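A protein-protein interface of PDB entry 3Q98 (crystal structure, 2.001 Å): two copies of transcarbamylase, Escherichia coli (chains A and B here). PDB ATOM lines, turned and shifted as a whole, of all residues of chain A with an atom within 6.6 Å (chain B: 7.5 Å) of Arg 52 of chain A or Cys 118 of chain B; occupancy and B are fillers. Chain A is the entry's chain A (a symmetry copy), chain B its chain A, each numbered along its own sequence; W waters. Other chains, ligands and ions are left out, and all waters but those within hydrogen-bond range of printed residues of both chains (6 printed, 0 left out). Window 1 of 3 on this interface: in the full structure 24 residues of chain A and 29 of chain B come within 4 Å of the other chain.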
ATOM      1  N   ALA A  47      32.785   2.223   5.299  1.00  0.00           N
ATOM      2  CA  ALA A  47      32.247   2.246   6.650  1.00  0.00           C
ATOM      3  C   ALA A  47      30.764   2.591   6.649  1.00  0.00           C
ATOM      4  O   ALA A  47      29.988   1.962   7.351  1.00  0.00           O
ATOM      5  CB  ALA A  47      33.024   3.197   7.535  1.00  0.00           C
ATOM      6  N   LEU A  48      30.360   3.573   5.849  1.00  0.00           N
ATOM      7  CA  LEU A  48      28.943   3.911   5.783  1.00  0.00           C
ATOM      8  C   LEU A  48      28.136   2.724   5.253  1.00  0.00           C
ATOM      9  O   LEU A  48      27.082   2.422   5.780  1.00  0.00           O
ATOM     10  CB  LEU A  48      28.691   5.147   4.929  1.00  0.00           C
ATOM     11  CG  LEU A  48      29.297   6.479   5.384  1.00  0.00           C
ATOM     12  CD1 LEU A  48      29.206   7.505   4.253  1.00  0.00           C
ATOM     13  CD2 LEU A  48      28.620   7.009   6.640  1.00  0.00           C
ATOM     14  N   LYS A  49      28.635   2.048   4.221  1.00  0.00           N
ATOM     15  CA  LYS A  49      27.892   0.928   3.640  1.00  0.00           C
ATOM     16  C   LYS A  49      27.717  -0.181   4.683  1.00  0.00           C
ATOM     17  O   LYS A  49      26.638  -0.765   4.807  1.00  0.00           O
ATOM     18  CB  LYS A  49      28.623   0.403   2.394  1.00  0.00           C
ATOM     19  CG  LYS A  49      27.793  -0.465   1.427  1.00  0.00           C
ATOM     20  CD  LYS A  49      28.505  -0.536   0.048  1.00  0.00           C
ATOM     21  CE  LYS A  49      27.679  -1.239  -1.026  1.00  0.00           C
ATOM     22  NZ  LYS A  49      27.442  -2.670  -0.670  1.00  0.00           N
ATOM     23  N   ALA A  50      28.790  -0.486   5.418  1.00  0.00           N
ATOM     24  CA  ALA A  50      28.745  -1.516   6.461  1.00  0.00           C
ATOM     25  C   ALA A  50      27.819  -1.121   7.614  1.00  0.00           C
ATOM     26  O   ALA A  50      27.045  -1.939   8.112  1.00  0.00           O
ATOM     27  CB  ALA A  50      30.140  -1.819   6.978  1.00  0.00           C
ATOM     28  N   LEU A  51      27.880   0.134   8.043  1.00  0.00           N
ATOM     29  CA  LEU A  51      26.947   0.575   9.081  1.00  0.00           C
ATOM     30  C   LEU A  51      25.497   0.381   8.639  1.00  0.00           C
ATOM     31  O   LEU A  51      24.667  -0.156   9.374  1.00  0.00           O
ATOM     32  CB  LEU A  51      27.187   2.038   9.432  1.00  0.00           C
ATOM     33  CG  LEU A  51      28.488   2.318  10.181  1.00  0.00           C
ATOM     34  CD1 LEU A  51      28.742   3.812  10.259  1.00  0.00           C
ATOM     35  CD2 LEU A  51      28.444   1.700  11.579  1.00  0.00           C
ATOM     36  N   ARG A  52      25.212   0.823   7.426  1.00  0.00           N
ATOM     37  CA  ARG A  52      23.877   0.777   6.860  1.00  0.00           C
ATOM     38  C   ARG A  52      23.396  -0.665   6.766  1.00  0.00           C
ATOM     39  O   ARG A  52      22.239  -0.958   7.062  1.00  0.00           O
ATOM     40  CB  ARG A  52      23.911   1.450   5.488  1.00  0.00           C
ATOM     41  CG  ARG A  52      22.628   1.418   4.665  1.00  0.00           C
ATOM     42  CD  ARG A  52      21.512   2.165   5.320  1.00  0.00           C
ATOM     43  NE  ARG A  52      20.450   2.523   4.379  1.00  0.00           N
ATOM     44  CZ  ARG A  52      19.692   1.646   3.724  1.00  0.00           C
ATOM     45  NH1 ARG A  52      19.895   0.344   3.874  1.00  0.00           N
ATOM     46  NH2 ARG A  52      18.736   2.075   2.912  1.00  0.00           N
ATOM     47  N   ALA A  53      24.303  -1.560   6.384  1.00  0.00           N
ATOM     48  CA  ALA A  53      24.007  -2.987   6.230  1.00  0.00           C
ATOM     49  C   ALA A  53      23.542  -3.647   7.522  1.00  0.00           C
ATOM     50  O   ALA A  53      22.734  -4.577   7.494  1.00  0.00           O
ATOM     51  CB  ALA A  53      25.227  -3.727   5.672  1.00  0.00           C
ATOM     52  N   GLU A  54      24.048  -3.172   8.655  1.00  0.00           N
ATOM     53  CA  GLU A  54      23.655  -3.741   9.940  1.00  0.00           C
ATOM     54  C   GLU A  54      22.659  -2.850  10.693  1.00  0.00           C
ATOM     55  O   GLU A  54      22.588  -2.884  11.926  1.00  0.00           O
ATOM     56  CB  GLU A  54      24.886  -4.040  10.799  1.00  0.00           C
ATOM     57  CG  GLU A  54      25.749  -5.191  10.271  1.00  0.00           C
ATOM     58  CD  GLU A  54      24.970  -6.487  10.122  1.00  0.00           C
ATOM     59  OE1 GLU A  54      25.108  -7.148   9.070  1.00  0.00           O
ATOM     60  OE2 GLU A  54      24.211  -6.843  11.049  1.00  0.00           O
ATOM     61  N   ASN A  55      21.912  -2.045   9.945  1.00  0.00           N
ATOM     62  CA  ASN A  55      20.819  -1.251  10.513  1.00  0.00           C
ATOM     63  C   ASN A  55      21.272  -0.182  11.508  1.00  0.00           C
ATOM     64  O   ASN A  55      20.546   0.148  12.443  1.00  0.00           O
ATOM     65  CB  ASN A  55      19.791  -2.167  11.188  1.00  0.00           C
ATOM     66  CG  ASN A  55      18.478  -1.467  11.438  1.00  0.00           C
ATOM     67  OD1 ASN A  55      18.117  -0.552  10.701  1.00  0.00           O
ATOM     68  ND2 ASN A  55      17.745  -1.900  12.472  1.00  0.00           N
ATOM     69  N   ILE A  56      22.476   0.349  11.319  1.00  0.00           N
ATOM     70  CA  ILE A  56      22.942   1.456  12.149  1.00  0.00           C
ATOM     71  C   ILE A  56      22.791   2.773  11.389  1.00  0.00           C
ATOM     72  O   ILE A  56      23.263   2.914  10.270  1.00  0.00           O
ATOM     73  CB  ILE A  56      24.403   1.270  12.611  1.00  0.00           C
ATOM     74  CG1 ILE A  56      24.489   0.137  13.637  1.00  0.00           C
ATOM     75  CG2 ILE A  56      24.948   2.583  13.192  1.00  0.00           C
ATOM     76  CD1 ILE A  56      25.882  -0.113  14.193  1.00  0.00           C
ATOM     77  N   SER A  57      22.119   3.730  12.012  1.00  0.00           N
ATOM     78  CA  SER A  57      21.859   5.019  11.399  1.00  0.00           C
ATOM     79  C   SER A  57      23.146   5.796  11.177  1.00  0.00           C
ATOM     80  O   SER A  57      23.999   5.872  12.061  1.00  0.00           O
ATOM     81  CB  SER A  57      20.951   5.839  12.320  1.00  0.00           C
ATOM     82  OG  SER A  57      20.821   7.171  11.856  1.00  0.00           O
ATOM     83  N   THR A  58      23.276   6.390  10.000  1.00  0.00           N
ATOM     84  CA  THR A  58      24.409   7.260   9.725  1.00  0.00           C
ATOM     85  C   THR A  58      23.940   8.717   9.548  1.00  0.00           C
ATOM     86  O   THR A  58      24.552   9.515   8.844  1.00  0.00           O
ATOM     87  CB  THR A  58      25.191   6.756   8.505  1.00  0.00           C
ATOM     88  OG1 THR A  58      26.389   7.522   8.363  1.00  0.00           O
ATOM     89  CG2 THR A  58      24.354   6.864   7.245  1.00  0.00           C
ATOM     90  N   SER A  83      19.863   9.616  -2.639  1.00  0.00           N
ATOM     91  CA  SER A  83      20.096   8.524  -1.702  1.00  0.00           C
ATOM     92  C   SER A  83      21.176   8.906  -0.714  1.00  0.00           C
ATOM     93  O   SER A  83      21.051   8.643   0.481  1.00  0.00           O
ATOM     94  CB  SER A  83      20.521   7.232  -2.436  1.00  0.00           C
ATOM     95  OG  SER A  83      19.537   6.803  -3.360  1.00  0.00           O
ATOM     96  N   ALA A  84      22.256   9.506  -1.216  1.00  0.00           N
ATOM     97  CA  ALA A  84      23.344   9.913  -0.337  1.00  0.00           C
ATOM     98  C   ALA A  84      22.890  10.992   0.656  1.00  0.00           C
ATOM     99  O   ALA A  84      23.231  10.957   1.831  1.00  0.00           O
ATOM    100  CB  ALA A  84      24.541  10.390  -1.140  1.00  0.00           C
ATOM    101  N   ASN A  86      19.928  11.517   1.769  1.00  0.00           N
ATOM    102  CA  ASN A  86      18.989  10.960   2.722  1.00  0.00           C
ATOM    103  C   ASN A  86      19.670  10.082   3.773  1.00  0.00           C
ATOM    104  O   ASN A  86      19.294  10.090   4.956  1.00  0.00           O
ATOM    105  CB  ASN A  86      17.904  10.187   1.989  1.00  0.00           C
ATOM    106  CG  ASN A  86      16.863   9.644   2.927  1.00  0.00           C
ATOM    107  OD1 ASN A  86      15.939  10.364   3.363  1.00  0.00           O
ATOM    108  ND2 ASN A  86      17.003   8.376   3.258  1.00  0.00           N
ATOM    109  N   LEU A  87      20.666   9.325   3.325  1.00  0.00           N
ATOM    110  CA  LEU A  87      21.531   8.538   4.196  1.00  0.00           C
ATOM    111  C   LEU A  87      22.128   9.373   5.340  1.00  0.00           C
ATOM    112  O   LEU A  87      22.284   8.887   6.464  1.00  0.00           O
ATOM    113  CB  LEU A  87      22.668   7.943   3.361  1.00  0.00           C
ATOM    114  CG  LEU A  87      23.344   6.683   3.880  1.00  0.00           C
ATOM    115  CD1 LEU A  87      22.388   5.502   3.788  1.00  0.00           C
ATOM    116  CD2 LEU A  87      24.624   6.411   3.099  1.00  0.00           C
ATOM    117  N   SER A 365      25.595   0.078  -6.631  1.00  0.00           N
ATOM    118  CA  SER A 365      25.219   0.218  -5.213  1.00  0.00           C
ATOM    119  C   SER A 365      26.225   1.047  -4.413  1.00  0.00           C
ATOM    120  O   SER A 365      25.904   1.556  -3.326  1.00  0.00           O
ATOM    121  CB  SER A 365      25.030  -1.164  -4.540  1.00  0.00           C
ATOM    122  OG  SER A 365      26.290  -1.781  -4.263  1.00  0.00           O
ATOM    123  N   PRO A 368      25.905   5.850  -3.855  1.00  0.00           N
ATOM    124  CA  PRO A 368      25.356   6.674  -2.757  1.00  0.00           C
ATOM    125  C   PRO A 368      26.360   6.813  -1.608  1.00  0.00           C
ATOM    126  O   PRO A 368      26.490   7.874  -0.995  1.00  0.00           O
ATOM    127  CB  PRO A 368      24.141   5.855  -2.278  1.00  0.00           C
ATOM    128  CG  PRO A 368      23.720   5.074  -3.468  1.00  0.00           C
ATOM    129  CD  PRO A 368      25.011   4.740  -4.216  1.00  0.00           C
ATOM    130  N   TYR A 369      27.090   5.735  -1.335  1.00  0.00           N
ATOM    131  CA  TYR A 369      28.077   5.753  -0.265  1.00  0.00           C
ATOM    132  C   TYR A 369      29.283   6.597  -0.595  1.00  0.00           C
ATOM    133  O   TYR A 369      29.841   7.231   0.284  1.00  0.00           O
ATOM    134  CB  TYR A 369      28.478   4.326   0.106  1.00  0.00           C
ATOM    135  CG  TYR A 369      27.256   3.542   0.459  1.00  0.00           C
ATOM    136  CD1 TYR A 369      26.641   2.716  -0.479  1.00  0.00           C
ATOM    137  CD2 TYR A 369      26.655   3.689   1.703  1.00  0.00           C
ATOM    138  CE1 TYR A 369      25.493   2.019  -0.162  1.00  0.00           C
ATOM    139  CE2 TYR A 369      25.519   2.986   2.027  1.00  0.00           C
ATOM    140  CZ  TYR A 369      24.938   2.167   1.094  1.00  0.00           C
ATOM    141  OH  TYR A 369      23.801   1.473   1.424  1.00  0.00           O
ATOM    142  N   ARG A 397      18.425   2.272  12.223  1.00  0.00           N
ATOM    143  CA  ARG A 397      17.812   2.964  11.098  1.00  0.00           C
ATOM    144  C   ARG A 397      16.327   2.649  11.052  1.00  0.00           C
ATOM    145  O   ARG A 397      15.501   3.550  10.920  1.00  0.00           O
ATOM    146  CB  ARG A 397      18.456   2.592   9.764  1.00  0.00           C
ATOM    147  CG  ARG A 397      17.852   3.376   8.601  1.00  0.00           C
ATOM    148  CD  ARG A 397      18.355   2.902   7.250  1.00  0.00           C
ATOM    149  NE  ARG A 397      17.363   2.073   6.554  1.00  0.00           N
ATOM    150  CZ  ARG A 397      17.542   0.795   6.255  1.00  0.00           C
ATOM    151  NH1 ARG A 397      18.677   0.194   6.597  1.00  0.00           N
ATOM    152  NH2 ARG A 397      16.598   0.117   5.611  1.00  0.00           N
ATOM    153  N   SER B  63      16.096   6.886   8.268  1.00  0.00           N
ATOM    154  CA  SER B  63      16.429   7.315   6.920  1.00  0.00           C
ATOM    155  C   SER B  63      15.882   6.225   6.020  1.00  0.00           C
ATOM    156  O   SER B  63      15.423   5.195   6.517  1.00  0.00           O
ATOM    157  CB  SER B  63      17.937   7.485   6.741  1.00  0.00           C
ATOM    158  OG  SER B  63      18.576   6.248   6.489  1.00  0.00           O
ATOM    159  N   GLY B  64      15.907   6.454   4.712  1.00  0.00           N
ATOM    160  CA  GLY B  64      15.282   5.552   3.762  1.00  0.00           C
ATOM    161  C   GLY B  64      14.412   6.311   2.776  1.00  0.00           C
ATOM    162  O   GLY B  64      13.816   7.331   3.118  1.00  0.00           O
ATOM    163  N   LEU B  65      14.353   5.803   1.547  1.00  0.00           N
ATOM    164  CA  LEU B  65      13.566   6.388   0.463  1.00  0.00           C
ATOM    165  C   LEU B  65      12.295   5.593   0.152  1.00  0.00           C
ATOM    166  O   LEU B  65      12.251   4.363   0.315  1.00  0.00           O
ATOM    167  CB  LEU B  65      14.427   6.454  -0.815  1.00  0.00           C
ATOM    168  CG  LEU B  65      15.085   7.769  -1.223  1.00  0.00           C
ATOM    169  CD1 LEU B  65      15.485   8.573  -0.025  1.00  0.00           C
ATOM    170  CD2 LEU B  65      16.251   7.570  -2.204  1.00  0.00           C
ATOM    171  N   GLY B  66      11.262   6.302  -0.301  1.00  0.00           N
ATOM    172  CA  GLY B  66      10.129   5.669  -0.955  1.00  0.00           C
ATOM    173  C   GLY B  66      10.078   6.194  -2.380  1.00  0.00           C
ATOM    174  O   GLY B  66       9.964   7.396  -2.596  1.00  0.00           O
ATOM    175  N   ILE B  67      10.162   5.306  -3.358  1.00  0.00           N
ATOM    176  CA  ILE B  67      10.222   5.732  -4.762  1.00  0.00           C
ATOM    177  C   ILE B  67       8.823   5.747  -5.368  1.00  0.00           C
ATOM    178  O   ILE B  67       8.020   4.878  -5.063  1.00  0.00           O
ATOM    179  CB  ILE B  67      11.110   4.788  -5.593  1.00  0.00           C
ATOM    180  CG1 ILE B  67      12.441   4.542  -4.881  1.00  0.00           C
ATOM    181  CG2 ILE B  67      11.382   5.372  -6.967  1.00  0.00           C
ATOM    182  CD1 ILE B  67      13.302   5.765  -4.738  1.00  0.00           C
ATOM    183  N   LEU B  90       9.981   8.002   5.889  1.00  0.00           N
ATOM    184  CA  LEU B  90      10.668   7.837   4.601  1.00  0.00           C
ATOM    185  C   LEU B  90      10.521   9.096   3.754  1.00  0.00           C
ATOM    186  O   LEU B  90       9.507   9.785   3.838  1.00  0.00           O
ATOM    187  CB  LEU B  90      10.085   6.637   3.831  1.00  0.00           C
ATOM    188  CG  LEU B  90      10.267   5.264   4.466  1.00  0.00           C
ATOM    189  CD1 LEU B  90       9.462   4.235   3.676  1.00  0.00           C
ATOM    190  CD2 LEU B  90      11.759   4.884   4.540  1.00  0.00           C
ATOM    191  N   ALA B  91      11.527   9.379   2.929  1.00  0.00           N
ATOM    192  CA  ALA B  91      11.499  10.517   2.025  1.00  0.00           C
ATOM    193  C   ALA B  91      11.059  10.067   0.633  1.00  0.00           C
ATOM    194  O   ALA B  91      11.511   9.029   0.138  1.00  0.00           O
ATOM    195  CB  ALA B  91      12.879  11.163   1.964  1.00  0.00           C
ATOM    196  N   ASN B 113      16.079  -2.660  -9.487  1.00  0.00           N
ATOM    197  CA  ASN B 113      17.273  -2.734  -8.651  1.00  0.00           C
ATOM    198  C   ASN B 113      17.952  -1.369  -8.507  1.00  0.00           C
ATOM    199  O   ASN B 113      18.316  -0.957  -7.405  1.00  0.00           O
ATOM    200  CB  ASN B 113      18.247  -3.788  -9.189  1.00  0.00           C
ATOM    201  CG  ASN B 113      17.887  -5.193  -8.734  1.00  0.00           C
ATOM    202  OD1 ASN B 113      18.379  -5.665  -7.711  1.00  0.00           O
ATOM    203  ND2 ASN B 113      17.020  -5.864  -9.489  1.00  0.00           N
ATOM    204  N   MET B 114      18.086  -0.673  -9.631  1.00  0.00           N
ATOM    205  CA  MET B 114      18.769   0.618  -9.714  1.00  0.00           C
ATOM    206  C   MET B 114      18.198   1.661  -8.739  1.00  0.00           C
ATOM    207  O   MET B 114      18.933   2.475  -8.177  1.00  0.00           O
ATOM    208  CB  MET B 114      18.669   1.140 -11.148  1.00  0.00           C
ATOM    209  CG  MET B 114      19.474   2.408 -11.436  1.00  0.00           C
ATOM    210  SD  MET B 114      19.158   3.079 -13.256  1.00  0.00           S
ATOM    211  CE  MET B 114      19.289   1.377 -14.222  1.00  0.00           C
ATOM    212  N   ILE B 115      16.890   1.616  -8.530  1.00  0.00           N
ATOM    213  CA  ILE B 115      16.224   2.596  -7.679  1.00  0.00           C
ATOM    214  C   ILE B 115      16.084   2.160  -6.215  1.00  0.00           C
ATOM    215  O   ILE B 115      15.580   2.924  -5.393  1.00  0.00           O
ATOM    216  CB  ILE B 115      14.815   2.935  -8.221  1.00  0.00           C
ATOM    217  CG1 ILE B 115      13.848   1.769  -7.957  1.00  0.00           C
ATOM    218  CG2 ILE B 115      14.896   3.293  -9.704  1.00  0.00           C
ATOM    219  CD1 ILE B 115      12.408   1.982  -8.460  1.00  0.00           C
ATOM    220  N   SER B 116      16.526   0.947  -5.889  1.00  0.00           N
ATOM    221  CA  SER B 116      16.173   0.347  -4.601  1.00  0.00           C
ATOM    222  C   SER B 116      17.281   0.230  -3.561  1.00  0.00           C
ATOM    223  O   SER B 116      17.034  -0.270  -2.461  1.00  0.00           O
ATOM    224  CB  SER B 116      15.562  -1.042  -4.829  1.00  0.00           C
ATOM    225  OG  SER B 116      14.319  -0.920  -5.497  1.00  0.00           O
ATOM    226  N   PHE B 117      18.498   0.653  -3.894  1.00  0.00           N
ATOM    227  CA  PHE B 117      19.613   0.519  -2.956  1.00  0.00           C
ATOM    228  C   PHE B 117      19.325   1.106  -1.574  1.00  0.00           C
ATOM    229  O   PHE B 117      19.718   0.535  -0.554  1.00  0.00           O
ATOM    230  CB  PHE B 117      20.878   1.155  -3.521  1.00  0.00           C
ATOM    231  CG  PHE B 117      21.271   0.626  -4.867  1.00  0.00           C
ATOM    232  CD1 PHE B 117      21.449  -0.734  -5.063  1.00  0.00           C
ATOM    233  CD2 PHE B 117      21.474   1.495  -5.936  1.00  0.00           C
ATOM    234  CE1 PHE B 117      21.822  -1.233  -6.316  1.00  0.00           C
ATOM    235  CE2 PHE B 117      21.842   1.007  -7.185  1.00  0.00           C
ATOM    236  CZ  PHE B 117      22.019  -0.354  -7.371  1.00  0.00           C
ATOM    237  N   CYS B 118      18.638   2.241  -1.551  1.00  0.00           N
ATOM    238  CA  CYS B 118      18.302   2.911  -0.302  1.00  0.00           C
ATOM    239  C   CYS B 118      16.796   3.087  -0.152  1.00  0.00           C
ATOM    240  O   CYS B 118      16.349   3.945   0.600  1.00  0.00           O
ATOM    241  CB  CYS B 118      18.980   4.288  -0.238  1.00  0.00           C
ATOM    242  SG  CYS B 118      20.785   4.212  -0.218  1.00  0.00           S
ATOM    243  N   ALA B 119      16.019   2.298  -0.887  1.00  0.00           N
ATOM    244  CA  ALA B 119      14.552   2.391  -0.815  1.00  0.00           C
ATOM    245  C   ALA B 119      13.950   1.346   0.104  1.00  0.00           C
ATOM    246  O   ALA B 119      14.296   0.174   0.033  1.00  0.00           O
ATOM    247  CB  ALA B 119      13.938   2.261  -2.191  1.00  0.00           C
ATOM    248  N   ASP B 120      13.036   1.766   0.960  1.00  0.00           N
ATOM    249  CA  ASP B 120      12.293   0.793   1.737  1.00  0.00           C
ATOM    250  C   ASP B 120      10.893   0.610   1.170  1.00  0.00           C
ATOM    251  O   ASP B 120      10.157  -0.284   1.592  1.00  0.00           O
ATOM    252  CB  ASP B 120      12.270   1.170   3.210  1.00  0.00           C
ATOM    253  CG  ASP B 120      13.654   1.106   3.833  1.00  0.00           C
ATOM    254  OD1 ASP B 120      14.112  -0.006   4.173  1.00  0.00           O
ATOM    255  OD2 ASP B 120      14.287   2.168   3.947  1.00  0.00           O
ATOM    256  N   ALA B 121      10.543   1.429   0.182  1.00  0.00           N
ATOM    257  CA  ALA B 121       9.247   1.281  -0.480  1.00  0.00           C
ATOM    258  C   ALA B 121       9.298   1.767  -1.911  1.00  0.00           C
ATOM    259  O   ALA B 121      10.027   2.702  -2.233  1.00  0.00           O
ATOM    260  CB  ALA B 121       8.151   2.014   0.298  1.00  0.00           C
ATOM    261  N   LEU B 153      20.607  -5.710  -2.712  1.00  0.00           N
ATOM    262  CA  LEU B 153      19.791  -4.821  -1.899  1.00  0.00           C
ATOM    263  C   LEU B 153      19.861  -5.263  -0.439  1.00  0.00           C
ATOM    264  O   LEU B 153      19.635  -6.432  -0.125  1.00  0.00           O
ATOM    265  CB  LEU B 153      18.343  -4.859  -2.390  1.00  0.00           C
ATOM    266  CG  LEU B 153      18.124  -4.737  -3.900  1.00  0.00           C
ATOM    267  CD1 LEU B 153      16.634  -4.804  -4.251  1.00  0.00           C
ATOM    268  CD2 LEU B 153      18.720  -3.436  -4.410  1.00  0.00           C
ATOM    269  N   PRO B 154      20.186  -4.326   0.460  1.00  0.00           N
ATOM    270  CA  PRO B 154      20.292  -4.606   1.897  1.00  0.00           C
ATOM    271  C   PRO B 154      18.909  -4.827   2.526  1.00  0.00           C
ATOM    272  O   PRO B 154      18.811  -5.421   3.594  1.00  0.00           O
ATOM    273  CB  PRO B 154      20.921  -3.328   2.469  1.00  0.00           C
ATOM    274  CG  PRO B 154      21.390  -2.528   1.270  1.00  0.00           C
ATOM    275  CD  PRO B 154      20.502  -2.927   0.139  1.00  0.00           C
ATOM    276  N   GLN B 155      17.869  -4.324   1.867  1.00  0.00           N
ATOM    277  CA  GLN B 155      16.482  -4.575   2.258  1.00  0.00           C
ATOM    278  C   GLN B 155      15.668  -4.900   1.008  1.00  0.00           C
ATOM    279  O   GLN B 155      16.009  -4.469  -0.094  1.00  0.00           O
ATOM    280  CB  GLN B 155      15.870  -3.358   2.963  1.00  0.00           C
ATOM    281  CG  GLN B 155      15.627  -2.167   2.035  1.00  0.00           C
ATOM    282  CD  GLN B 155      16.930  -1.484   1.636  1.00  0.00           C
ATOM    283  OE1 GLN B 155      17.738  -1.139   2.494  1.00  0.00           O
ATOM    284  NE2 GLN B 155      17.139  -1.296   0.334  1.00  0.00           N
ATOM    285  N   PRO B 157      12.519  -3.870  -0.710  1.00  0.00           N
ATOM    286  CA  PRO B 157      11.522  -2.801  -0.571  1.00  0.00           C
ATOM    287  C   PRO B 157      10.096  -3.329  -0.584  1.00  0.00           C
ATOM    288  O   PRO B 157       9.811  -4.282  -1.297  1.00  0.00           O
ATOM    289  CB  PRO B 157      11.726  -1.954  -1.828  1.00  0.00           C
ATOM    290  CG  PRO B 157      13.063  -2.279  -2.314  1.00  0.00           C
ATOM    291  CD  PRO B 157      13.314  -3.715  -1.939  1.00  0.00           C
HETATM  292  O   HOH W   1      19.537   6.934   9.649  1.00  0.00           O
HETATM  293  O   HOH W   2      13.923   9.031   5.377  1.00  0.00           O
HETATM  294  O   HOH W   3      22.502   0.191  -0.493  1.00  0.00           O
HETATM  295  O   HOH W   4      17.636   4.030  -3.555  1.00  0.00           O
HETATM  296  O   HOH W   5      21.022   6.595   7.733  1.00  0.00           O
HETATM  297  O   HOH W   6      18.951   5.098   4.015  1.00  0.00           O
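N of Gly 64 of chain B lies close to ND2 of Asn 86 of chain A, 2.6 Å away. OD1 of Asp 120 of chain B lies within salt-bridge range of NH2 of Arg 397 of chain A (2.9 Å). The side-chain amide oxygen (OE1) of Gln 155 of chain B lies within hydrogen-bond range of the guanidinium group (NH1) of Arg 52 of chain A (3.0 Å).
The backbone NH of Leu 65 of chain B lies within hydrogen-bond range of the backbone carbonyl oxygen of Cys 118 of chain B (2.9 Å). N of Asp 120 of chain B lies within hydrogen-bond range of O of Leu 65 of chain B, 2.8 Å away. O of Leu 65 of chain B lies within hydrogen-bond range of N of Ala 121 of chain B (3.4 Å). O of Ser 116 of chain B sits at hydrogen-bond distance from NE2 of Gln 155 of chain B (3.0 Å). The backbone carbonyl oxygen (O) of Ala 119 of chain B sits at hydrogen-bond distance from the side-chain amide nitrogen (NE2) of Gln 155 of chain B (3.2 Å). The backbone NH (N) of Arg 397 of chain A sits at hydrogen-bond distance from the backbone carbonyl oxygen (O) of Asn 55 of chain A (3.0 Å).
Arg 52 of chain A touches Phe 117 of chain B. Cys 118 of chain B touches Arg 52 of chain A (CA to NH2, 3.3 Å). CD2 of Leu 65 of chain B touches OG of Ser 83 of chain A, 3.6 Å away. Ser 83 of chain A touches Cys 118 of chain B (CB to SG, 3.8 Å). Ser 63 of chain B touches Asn 86 of chain A (CB to O, 3.4 Å). CG of Asn 86 of chain A touches CD1 of Leu 65 of chain B, at 3.4 Å. OD1 of Asn 86 of chain A touches CB of Ala 91 of chain B, 3.5 Å away. Ser 365 of chain A touches Phe 117 of chain B (CB to CD1, 3.6 Å). Arg 397 of chain A touches Ser 63 of chain B. Gln 155 of chain B touches Arg 397 of chain A (OE1 to NH2, 3.5 Å).
Arg 52 of chain A touches just these residues of chain B: Phe 117 (3.9 Å), Cys 118 (3.3 Å) and Gln 155 (3.0 Å). Of chain A, only Arg 52 (3.3 Å) and Ser 83 (3.8 Å) come within 4 Å of Cys 118 of chain B. Printed residues of chain A within 4 Å of Asp 120 of chain B: Arg 397 (2.9 Å). Of the printed residues of chain B, Ser 83 of chain A touches Leu 65 and Cys 118. Of the printed residues of chain A, Gly 64 of chain B touches Asn 86 (2.6 Å). Of the printed residues of chain B, Ser 365 of chain A touches Phe 117 (3.6 Å). Ala 53 of chain A touches none of the printed residues of chain B. The nearest residue of chain B that does not touch Arg 52 of chain A is Pro 154 of chain B (4.1 Å).
Hydrophobic or aromatic side chains of chain B within 4 Å of the printed part of chain A: Leu 65, Ala 91 and Phe 117. Of the 20 printed residues of chain A, 5 touch a printed residue of chain B.
No position is printed for both chains.
Water W1 lies within hydrogen-bond range of the side-chain hydroxyl (OG) of Ser 57 of chain A and the side-chain hydroxyl (OG) of Ser 63 of chain B. Water W3 bridges OH of Tyr 369 of chain A (2.6 Å) and O of Phe 117 of chain B (2.8 Å). Water W6 lies within hydrogen-bond range of the side-chain hydroxyl (OG) of Ser 63 of chain B (2.8 Å), the guanidinium group (NE) of Arg 52 of chain A (3.0 Å) and the backbone NH (N) of Gly 64 of chain B (3.4 Å). Water W5 lies within hydrogen-bond range of the side-chain hydroxyl of Ser 63 of chain B (2.8 Å), the backbone carbonyl oxygen of Leu 87 of chain A (2.9 Å) and the backbone NH of Thr 58 of chain A (3.2 Å). Water W2 lies within hydrogen-bond range of O of Gly 64 of chain B, OD1 of Asn 86 of chain A and N of Ala 91 of chain B. Water W4 lies within hydrogen-bond range of the backbone NH of Cys 118 of chain B (2.9 Å), the backbone carbonyl oxygen of Ile 115 of chain B (3.0 Å) and the side-chain hydroxyl of Ser 83 of chain A (3.4 Å).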
